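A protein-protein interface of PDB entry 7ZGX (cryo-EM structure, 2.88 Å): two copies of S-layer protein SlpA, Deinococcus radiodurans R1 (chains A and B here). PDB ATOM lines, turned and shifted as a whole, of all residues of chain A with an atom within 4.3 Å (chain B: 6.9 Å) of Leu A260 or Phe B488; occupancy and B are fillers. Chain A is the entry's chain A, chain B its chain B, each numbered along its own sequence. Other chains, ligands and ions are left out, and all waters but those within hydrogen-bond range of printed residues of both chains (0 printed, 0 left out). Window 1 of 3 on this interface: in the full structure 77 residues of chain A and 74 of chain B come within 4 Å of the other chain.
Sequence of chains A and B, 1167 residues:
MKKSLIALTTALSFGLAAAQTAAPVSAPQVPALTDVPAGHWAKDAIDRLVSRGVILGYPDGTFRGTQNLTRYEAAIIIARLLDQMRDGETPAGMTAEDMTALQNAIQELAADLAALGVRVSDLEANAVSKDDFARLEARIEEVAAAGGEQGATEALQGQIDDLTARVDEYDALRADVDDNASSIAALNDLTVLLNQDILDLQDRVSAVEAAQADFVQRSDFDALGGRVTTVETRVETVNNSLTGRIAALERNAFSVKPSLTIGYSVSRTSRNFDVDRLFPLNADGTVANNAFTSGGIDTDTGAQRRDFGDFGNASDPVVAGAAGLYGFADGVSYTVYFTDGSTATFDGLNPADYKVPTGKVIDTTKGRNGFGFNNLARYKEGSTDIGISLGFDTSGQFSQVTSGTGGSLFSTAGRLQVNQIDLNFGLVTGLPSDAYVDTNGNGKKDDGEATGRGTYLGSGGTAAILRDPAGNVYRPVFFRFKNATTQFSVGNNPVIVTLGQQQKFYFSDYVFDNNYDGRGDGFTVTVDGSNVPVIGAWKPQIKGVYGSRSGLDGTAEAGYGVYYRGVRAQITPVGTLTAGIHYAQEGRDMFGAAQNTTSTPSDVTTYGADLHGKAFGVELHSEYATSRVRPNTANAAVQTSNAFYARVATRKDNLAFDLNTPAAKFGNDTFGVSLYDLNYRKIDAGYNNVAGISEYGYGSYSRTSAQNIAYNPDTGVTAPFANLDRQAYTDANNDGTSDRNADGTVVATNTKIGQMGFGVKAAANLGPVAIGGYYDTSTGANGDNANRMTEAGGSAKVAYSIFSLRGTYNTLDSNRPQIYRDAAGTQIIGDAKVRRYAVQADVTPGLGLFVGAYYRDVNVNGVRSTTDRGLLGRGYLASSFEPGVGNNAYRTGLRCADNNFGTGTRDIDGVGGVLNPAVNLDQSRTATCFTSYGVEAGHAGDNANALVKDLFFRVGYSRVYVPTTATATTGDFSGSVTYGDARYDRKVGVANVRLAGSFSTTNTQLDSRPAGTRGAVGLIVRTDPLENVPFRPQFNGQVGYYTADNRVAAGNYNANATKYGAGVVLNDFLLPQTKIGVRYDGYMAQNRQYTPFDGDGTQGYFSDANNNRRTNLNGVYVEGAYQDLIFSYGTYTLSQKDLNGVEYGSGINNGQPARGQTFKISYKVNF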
ATOM      1  N   SER A 259       3.420   5.602  -4.827  1.00  0.00           N
ATOM      2  CA  SER A 259       3.970   5.046  -6.048  1.00  0.00           C
ATOM      3  C   SER A 259       4.607   6.167  -6.847  1.00  0.00           C
ATOM      4  O   SER A 259       4.077   7.277  -6.936  1.00  0.00           O
ATOM      5  CB  SER A 259       2.900   4.334  -6.882  1.00  0.00           C
ATOM      6  OG  SER A 259       1.977   5.260  -7.420  1.00  0.00           O
ATOM      7  N   LEU A 260       5.758   5.854  -7.430  1.00  0.00           N
ATOM      8  CA  LEU A 260       6.527   6.827  -8.196  1.00  0.00           C
ATOM      9  C   LEU A 260       6.873   6.203  -9.534  1.00  0.00           C
ATOM     10  O   LEU A 260       7.356   5.068  -9.578  1.00  0.00           O
ATOM     11  CB  LEU A 260       7.790   7.228  -7.448  1.00  0.00           C
ATOM     12  CG  LEU A 260       8.681   8.255  -8.137  1.00  0.00           C
ATOM     13  CD1 LEU A 260       8.006   9.602  -8.133  1.00  0.00           C
ATOM     14  CD2 LEU A 260      10.030   8.331  -7.457  1.00  0.00           C
ATOM     15  N   THR A 261       6.619   6.927 -10.616  1.00  0.00           N
ATOM     16  CA  THR A 261       6.951   6.468 -11.957  1.00  0.00           C
ATOM     17  C   THR A 261       7.904   7.461 -12.598  1.00  0.00           C
ATOM     18  O   THR A 261       7.620   8.659 -12.636  1.00  0.00           O
ATOM     19  CB  THR A 261       5.704   6.318 -12.827  1.00  0.00           C
ATOM     20  OG1 THR A 261       5.162   7.613 -13.107  1.00  0.00           O
ATOM     21  CG2 THR A 261       4.659   5.492 -12.112  1.00  0.00           C
ATOM     22  N   ILE A 262       9.022   6.962 -13.102  1.00  0.00           N
ATOM     23  CA  ILE A 262      10.015   7.764 -13.798  1.00  0.00           C
ATOM     24  C   ILE A 262      10.214   7.194 -15.194  1.00  0.00           C
ATOM     25  O   ILE A 262      10.326   5.976 -15.366  1.00  0.00           O
ATOM     26  CB  ILE A 262      11.339   7.821 -13.004  1.00  0.00           C
ATOM     27  CG1 ILE A 262      12.285   8.879 -13.570  1.00  0.00           C
ATOM     28  CG2 ILE A 262      11.984   6.465 -12.891  1.00  0.00           C
ATOM     29  CD1 ILE A 262      11.812  10.265 -13.437  1.00  0.00           C
ATOM     30  N   ILE A 386       7.722  12.324 -14.300  1.00  0.00           N
ATOM     31  CA  ILE A 386       7.617  11.847 -12.928  1.00  0.00           C
ATOM     32  C   ILE A 386       6.138  11.833 -12.577  1.00  0.00           C
ATOM     33  O   ILE A 386       5.452  12.855 -12.700  1.00  0.00           O
ATOM     34  CB  ILE A 386       8.396  12.729 -11.942  1.00  0.00           C
ATOM     35  CG1 ILE A 386       9.895  12.690 -12.210  1.00  0.00           C
ATOM     36  CG2 ILE A 386       8.128  12.290 -10.525  1.00  0.00           C
ATOM     37  CD1 ILE A 386      10.394  13.721 -13.175  1.00  0.00           C
ATOM     38  N   GLY A 387       5.646  10.681 -12.148  1.00  0.00           N
ATOM     39  CA  GLY A 387       4.277  10.558 -11.696  1.00  0.00           C
ATOM     40  C   GLY A 387       4.211  10.094 -10.261  1.00  0.00           C
ATOM     41  O   GLY A 387       4.726   9.023  -9.931  1.00  0.00           O
ATOM     42  N   ILE A 388       3.593  10.894  -9.398  1.00  0.00           N
ATOM     43  CA  ILE A 388       3.466  10.582  -7.982  1.00  0.00           C
ATOM     44  C   ILE A 388       2.015  10.251  -7.688  1.00  0.00           C
ATOM     45  O   ILE A 388       1.097  10.979  -8.082  1.00  0.00           O
ATOM     46  CB  ILE A 388       3.932  11.737  -7.073  1.00  0.00           C
ATOM     47  CG1 ILE A 388       5.380  12.113  -7.361  1.00  0.00           C
ATOM     48  CG2 ILE A 388       3.772  11.360  -5.621  1.00  0.00           C
ATOM     49  CD1 ILE A 388       5.514  13.275  -8.300  1.00  0.00           C
ATOM     50  N   VAL A1165      10.768   1.896  -9.991  1.00  0.00           N
ATOM     51  CA  VAL A1165      11.138   2.134  -8.603  1.00  0.00           C
ATOM     52  C   VAL A1165       9.950   1.796  -7.714  1.00  0.00           C
ATOM     53  O   VAL A1165       8.803   2.106  -8.054  1.00  0.00           O
ATOM     54  CB  VAL A1165      11.599   3.584  -8.374  1.00  0.00           C
ATOM     55  CG1 VAL A1165      12.887   3.843  -9.105  1.00  0.00           C
ATOM     56  CG2 VAL A1165      10.544   4.552  -8.842  1.00  0.00           C
ATOM     57  N   PHE A1167       8.585   1.920  -3.562  1.00  0.00           N
ATOM     58  CA  PHE A1167       8.826   2.493  -2.248  1.00  0.00           C
ATOM     59  C   PHE A1167       9.124   1.403  -1.228  1.00  0.00           C
ATOM     60  O   PHE A1167       8.922   1.593  -0.030  1.00  0.00           O
ATOM     61  CB  PHE A1167       7.631   3.321  -1.790  1.00  0.00           C
ATOM     62  CG  PHE A1167       7.713   4.758  -2.188  1.00  0.00           C
ATOM     63  CD1 PHE A1167       7.298   5.165  -3.436  1.00  0.00           C
ATOM     64  CD2 PHE A1167       8.221   5.700  -1.318  1.00  0.00           C
ATOM     65  CE1 PHE A1167       7.376   6.485  -3.804  1.00  0.00           C
ATOM     66  CE2 PHE A1167       8.301   7.018  -1.684  1.00  0.00           C
ATOM     67  CZ  PHE A1167       7.876   7.410  -2.927  1.00  0.00           C
ATOM     68  N   VAL B 401      13.638   4.746  -2.327  1.00  0.00           N
ATOM     69  CA  VAL B 401      13.025   3.942  -3.377  1.00  0.00           C
ATOM     70  C   VAL B 401      14.039   2.907  -3.840  1.00  0.00           C
ATOM     71  O   VAL B 401      15.232   3.202  -3.939  1.00  0.00           O
ATOM     72  CB  VAL B 401      12.536   4.793  -4.567  1.00  0.00           C
ATOM     73  CG1 VAL B 401      11.329   5.611  -4.180  1.00  0.00           C
ATOM     74  CG2 VAL B 401      13.629   5.697  -5.047  1.00  0.00           C
ATOM     75  N   ASN B 419      17.563   4.802  -4.364  1.00  0.00           N
ATOM     76  CA  ASN B 419      17.579   6.232  -4.615  1.00  0.00           C
ATOM     77  C   ASN B 419      16.905   6.986  -3.477  1.00  0.00           C
ATOM     78  O   ASN B 419      15.964   6.494  -2.846  1.00  0.00           O
ATOM     79  CB  ASN B 419      16.884   6.560  -5.934  1.00  0.00           C
ATOM     80  CG  ASN B 419      17.764   6.311  -7.129  1.00  0.00           C
ATOM     81  OD1 ASN B 419      17.374   5.624  -8.068  1.00  0.00           O
ATOM     82  ND2 ASN B 419      18.960   6.876  -7.104  1.00  0.00           N
ATOM     83  N   GLN B 420      17.402   8.196  -3.232  1.00  0.00           N
ATOM     84  CA  GLN B 420      16.905   9.089  -2.193  1.00  0.00           C
ATOM     85  C   GLN B 420      15.998  10.117  -2.852  1.00  0.00           C
ATOM     86  O   GLN B 420      16.429  10.836  -3.759  1.00  0.00           O
ATOM     87  CB  GLN B 420      18.060   9.778  -1.475  1.00  0.00           C
ATOM     88  CG  GLN B 420      19.045   8.834  -0.841  1.00  0.00           C
ATOM     89  CD  GLN B 420      18.507   8.222   0.422  1.00  0.00           C
ATOM     90  OE1 GLN B 420      17.914   8.908   1.250  1.00  0.00           O
ATOM     91  NE2 GLN B 420      18.704   6.920   0.579  1.00  0.00           N
ATOM     92  N   ILE B 421      14.752  10.189  -2.400  1.00  0.00           N
ATOM     93  CA  ILE B 421      13.817  11.174  -2.927  1.00  0.00           C
ATOM     94  C   ILE B 421      13.559  12.233  -1.866  1.00  0.00           C
ATOM     95  O   ILE B 421      13.975  12.084  -0.713  1.00  0.00           O
ATOM     96  CB  ILE B 421      12.509  10.514  -3.388  1.00  0.00           C
ATOM     97  CG1 ILE B 421      11.645  10.169  -2.185  1.00  0.00           C
ATOM     98  CG2 ILE B 421      12.797   9.271  -4.201  1.00  0.00           C
ATOM     99  CD1 ILE B 421      10.240   9.841  -2.550  1.00  0.00           C
ATOM    100  N   LEU B 423      10.274  13.725  -1.408  1.00  0.00           N
ATOM    101  CA  LEU B 423       8.827  13.877  -1.402  1.00  0.00           C
ATOM    102  C   LEU B 423       8.350  14.071   0.026  1.00  0.00           C
ATOM    103  O   LEU B 423       8.615  13.229   0.889  1.00  0.00           O
ATOM    104  CB  LEU B 423       8.152  12.649  -2.009  1.00  0.00           C
ATOM    105  CG  LEU B 423       6.683  12.770  -2.395  1.00  0.00           C
ATOM    106  CD1 LEU B 423       6.552  13.429  -3.745  1.00  0.00           C
ATOM    107  CD2 LEU B 423       6.028  11.405  -2.400  1.00  0.00           C
ATOM    108  N   ASN B 483       7.292  17.631  -4.312  1.00  0.00           N
ATOM    109  CA  ASN B 483       8.309  16.754  -4.875  1.00  0.00           C
ATOM    110  C   ASN B 483       9.461  17.609  -5.377  1.00  0.00           C
ATOM    111  O   ASN B 483       9.347  18.271  -6.413  1.00  0.00           O
ATOM    112  CB  ASN B 483       7.734  15.913  -6.010  1.00  0.00           C
ATOM    113  CG  ASN B 483       8.610  14.734  -6.354  1.00  0.00           C
ATOM    114  OD1 ASN B 483       9.266  14.163  -5.488  1.00  0.00           O
ATOM    115  ND2 ASN B 483       8.637  14.370  -7.628  1.00  0.00           N
ATOM    116  N   THR B 485      12.634  16.214  -5.800  1.00  0.00           N
ATOM    117  CA  THR B 485      13.596  15.353  -6.475  1.00  0.00           C
ATOM    118  C   THR B 485      13.213  15.197  -7.936  1.00  0.00           C
ATOM    119  O   THR B 485      12.086  14.803  -8.251  1.00  0.00           O
ATOM    120  CB  THR B 485      13.664  13.986  -5.805  1.00  0.00           C
ATOM    121  OG1 THR B 485      14.028  14.145  -4.429  1.00  0.00           O
ATOM    122  CG2 THR B 485      14.697  13.121  -6.493  1.00  0.00           C
ATOM    123  N   THR B 486      14.154  15.498  -8.829  1.00  0.00           N
ATOM    124  CA  THR B 486      13.938  15.296 -10.255  1.00  0.00           C
ATOM    125  C   THR B 486      15.144  14.649 -10.923  1.00  0.00           C
ATOM    126  O   THR B 486      15.268  14.714 -12.148  1.00  0.00           O
ATOM    127  CB  THR B 486      13.622  16.619 -10.951  1.00  0.00           C
ATOM    128  OG1 THR B 486      14.507  17.634 -10.469  1.00  0.00           O
ATOM    129  CG2 THR B 486      12.194  17.035 -10.673  1.00  0.00           C
ATOM    130  N   GLN B 487      16.039  14.035 -10.152  1.00  0.00           N
ATOM    131  CA  GLN B 487      17.245  13.413 -10.692  1.00  0.00           C
ATOM    132  C   GLN B 487      17.387  12.044 -10.044  1.00  0.00           C
ATOM    133  O   GLN B 487      17.267  11.924  -8.823  1.00  0.00           O
ATOM    134  CB  GLN B 487      18.481  14.265 -10.415  1.00  0.00           C
ATOM    135  CG  GLN B 487      18.371  15.707 -10.862  1.00  0.00           C
ATOM    136  CD  GLN B 487      18.663  15.889 -12.328  1.00  0.00           C
ATOM    137  OE1 GLN B 487      17.759  16.126 -13.125  1.00  0.00           O
ATOM    138  NE2 GLN B 487      19.932  15.776 -12.697  1.00  0.00           N
ATOM    139  N   PHE B 488      17.639  11.020 -10.847  1.00  0.00           N
ATOM    140  CA  PHE B 488      17.859   9.671 -10.343  1.00  0.00           C
ATOM    141  C   PHE B 488      19.163   9.143 -10.924  1.00  0.00           C
ATOM    142  O   PHE B 488      19.343   9.128 -12.144  1.00  0.00           O
ATOM    143  CB  PHE B 488      16.682   8.768 -10.693  1.00  0.00           C
ATOM    144  CG  PHE B 488      15.416   9.147  -9.994  1.00  0.00           C
ATOM    145  CD1 PHE B 488      14.597  10.131 -10.506  1.00  0.00           C
ATOM    146  CD2 PHE B 488      15.055   8.535  -8.812  1.00  0.00           C
ATOM    147  CE1 PHE B 488      13.437  10.487  -9.859  1.00  0.00           C
ATOM    148  CE2 PHE B 488      13.895   8.889  -8.162  1.00  0.00           C
ATOM    149  CZ  PHE B 488      13.087   9.866  -8.686  1.00  0.00           C
ATOM    150  N   SER B 489      20.065   8.704 -10.056  1.00  0.00           N
ATOM    151  CA  SER B 489      21.393   8.269 -10.463  1.00  0.00           C
ATOM    152  C   SER B 489      21.521   6.766 -10.255  1.00  0.00           C
ATOM    153  O   SER B 489      21.053   6.232  -9.246  1.00  0.00           O
ATOM    154  CB  SER B 489      22.467   9.015  -9.676  1.00  0.00           C
ATOM    155  OG  SER B 489      22.401   8.687  -8.303  1.00  0.00           O
ATOM    156  N   VAL B 490      22.143   6.092 -11.216  1.00  0.00           N
ATOM    157  CA  VAL B 490      22.326   4.653 -11.181  1.00  0.00           C
ATOM    158  C   VAL B 490      23.797   4.338 -11.422  1.00  0.00           C
ATOM    159  O   VAL B 490      24.435   4.889 -12.319  1.00  0.00           O
ATOM    160  CB  VAL B 490      21.433   3.951 -12.224  1.00  0.00           C
ATOM    161  CG1 VAL B 490      21.576   2.457 -12.115  1.00  0.00           C
ATOM    162  CG2 VAL B 490      19.992   4.362 -12.049  1.00  0.00           C
ATOM    163  N   ILE B 496      28.101   6.341 -13.788  1.00  0.00           N
ATOM    164  CA  ILE B 496      26.929   6.847 -13.090  1.00  0.00           C
ATOM    165  C   ILE B 496      26.030   7.509 -14.117  1.00  0.00           C
ATOM    166  O   ILE B 496      26.435   8.481 -14.764  1.00  0.00           O
ATOM    167  CB  ILE B 496      27.307   7.835 -11.980  1.00  0.00           C
ATOM    168  CG1 ILE B 496      27.954   7.090 -10.819  1.00  0.00           C
ATOM    169  CG2 ILE B 496      26.086   8.590 -11.512  1.00  0.00           C
ATOM    170  CD1 ILE B 496      28.564   7.994  -9.783  1.00  0.00           C
ATOM    171  N   VAL B 497      24.820   6.988 -14.270  1.00  0.00           N
ATOM    172  CA  VAL B 497      23.860   7.496 -15.240  1.00  0.00           C
ATOM    173  C   VAL B 497      22.755   8.222 -14.496  1.00  0.00           C
ATOM    174  O   VAL B 497      22.095   7.652 -13.625  1.00  0.00           O
ATOM    175  CB  VAL B 497      23.279   6.366 -16.107  1.00  0.00           C
ATOM    176  CG1 VAL B 497      22.498   6.940 -17.260  1.00  0.00           C
ATOM    177  CG2 VAL B 497      24.384   5.475 -16.610  1.00  0.00           C
ATOM    178  N   THR B 498      22.548   9.488 -14.844  1.00  0.00           N
ATOM    179  CA  THR B 498      21.559  10.333 -14.191  1.00  0.00           C
ATOM    180  C   THR B 498      20.432  10.616 -15.167  1.00  0.00           C
ATOM    181  O   THR B 498      20.676  11.085 -16.279  1.00  0.00           O
ATOM    182  CB  THR B 498      22.187  11.641 -13.715  1.00  0.00           C
ATOM    183  OG1 THR B 498      23.216  11.359 -12.762  1.00  0.00           O
ATOM    184  CG2 THR B 498      21.142  12.525 -13.086  1.00  0.00           C
ATOM    185  N   LEU B 499      19.208  10.337 -14.747  1.00  0.00           N
ATOM    186  CA  LEU B 499      18.010  10.585 -15.533  1.00  0.00           C
ATOM    187  C   LEU B 499      17.197  11.671 -14.848  1.00  0.00           C
ATOM    188  O   LEU B 499      17.054  11.650 -13.623  1.00  0.00           O
ATOM    189  CB  LEU B 499      17.176   9.312 -15.653  1.00  0.00           C
ATOM    190  CG  LEU B 499      15.901   9.377 -16.485  1.00  0.00           C
ATOM    191  CD1 LEU B 499      16.219   9.674 -17.930  1.00  0.00           C
ATOM    192  CD2 LEU B 499      15.122   8.090 -16.354  1.00  0.00           C
ATOM    193  N   GLY B 500      16.665  12.613 -15.615  1.00  0.00           N
ATOM    194  CA  GLY B 500      15.737  13.529 -14.988  1.00  0.00           C
ATOM    195  C   GLY B 500      15.396  14.735 -15.831  1.00  0.00           C
ATOM    196  O   GLY B 500      15.831  14.882 -16.978  1.00  0.00           O
ATOM    197  N   GLN B 503      17.957  18.921 -16.825  1.00  0.00           N
ATOM    198  CA  GLN B 503      19.304  18.454 -16.549  1.00  0.00           C
ATOM    199  C   GLN B 503      20.265  19.631 -16.473  1.00  0.00           C
ATOM    200  O   GLN B 503      20.412  20.389 -17.434  1.00  0.00           O
ATOM    201  CB  GLN B 503      19.754  17.482 -17.636  1.00  0.00           C
ATOM    202  CG  GLN B 503      19.079  16.134 -17.586  1.00  0.00           C
ATOM    203  CD  GLN B 503      19.501  15.324 -16.389  1.00  0.00           C
ATOM    204  OE1 GLN B 503      18.684  14.658 -15.760  1.00  0.00           O
ATOM    205  NE2 GLN B 503      20.782  15.378 -16.063  1.00  0.00           N
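O of Phe B488 lies within hydrogen-bond range of N of Leu B499 (2.9 Å).
Among the printed residues, pairs that only touch across the chains: Leu A260 with Phe B488, Ile A262 with Phe B488, Ile A386 with Asn B483, Ile A388 with Leu B423, Ile A388 with Asn B483 and Phe A1167 with Ile B421.
Printed residues of chain B within 4 Å of Leu A260: Phe B488.
Of the printed residues of chain A, Leu B423 touches Ile A388.
Of the printed residues of chain B, Phe A1167 touches Ile B421 (3.4 Å).
Of the printed residues of chain B, Ile A388 touches Leu B423 (3.9 Å) and Asn B483 (3.4 Å).
Printed residues of chain A within 4 Å of Asn B483: Ile A386 (3.6 Å) and Ile A388 (3.4 Å).
Thr B486 touches none of the printed residues of chain A.
Ser A259 touches none of the printed residues of chain B.
Among the printed residues, no Asp or Glu carboxylate lies within 4 Å of a Lys or Arg side-chain nitrogen of the other chain.
No position is printed for both chains.
Of the 6 pairs that touch across the chains among the printed residues, none has its exchanged pair printed and touching as well.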
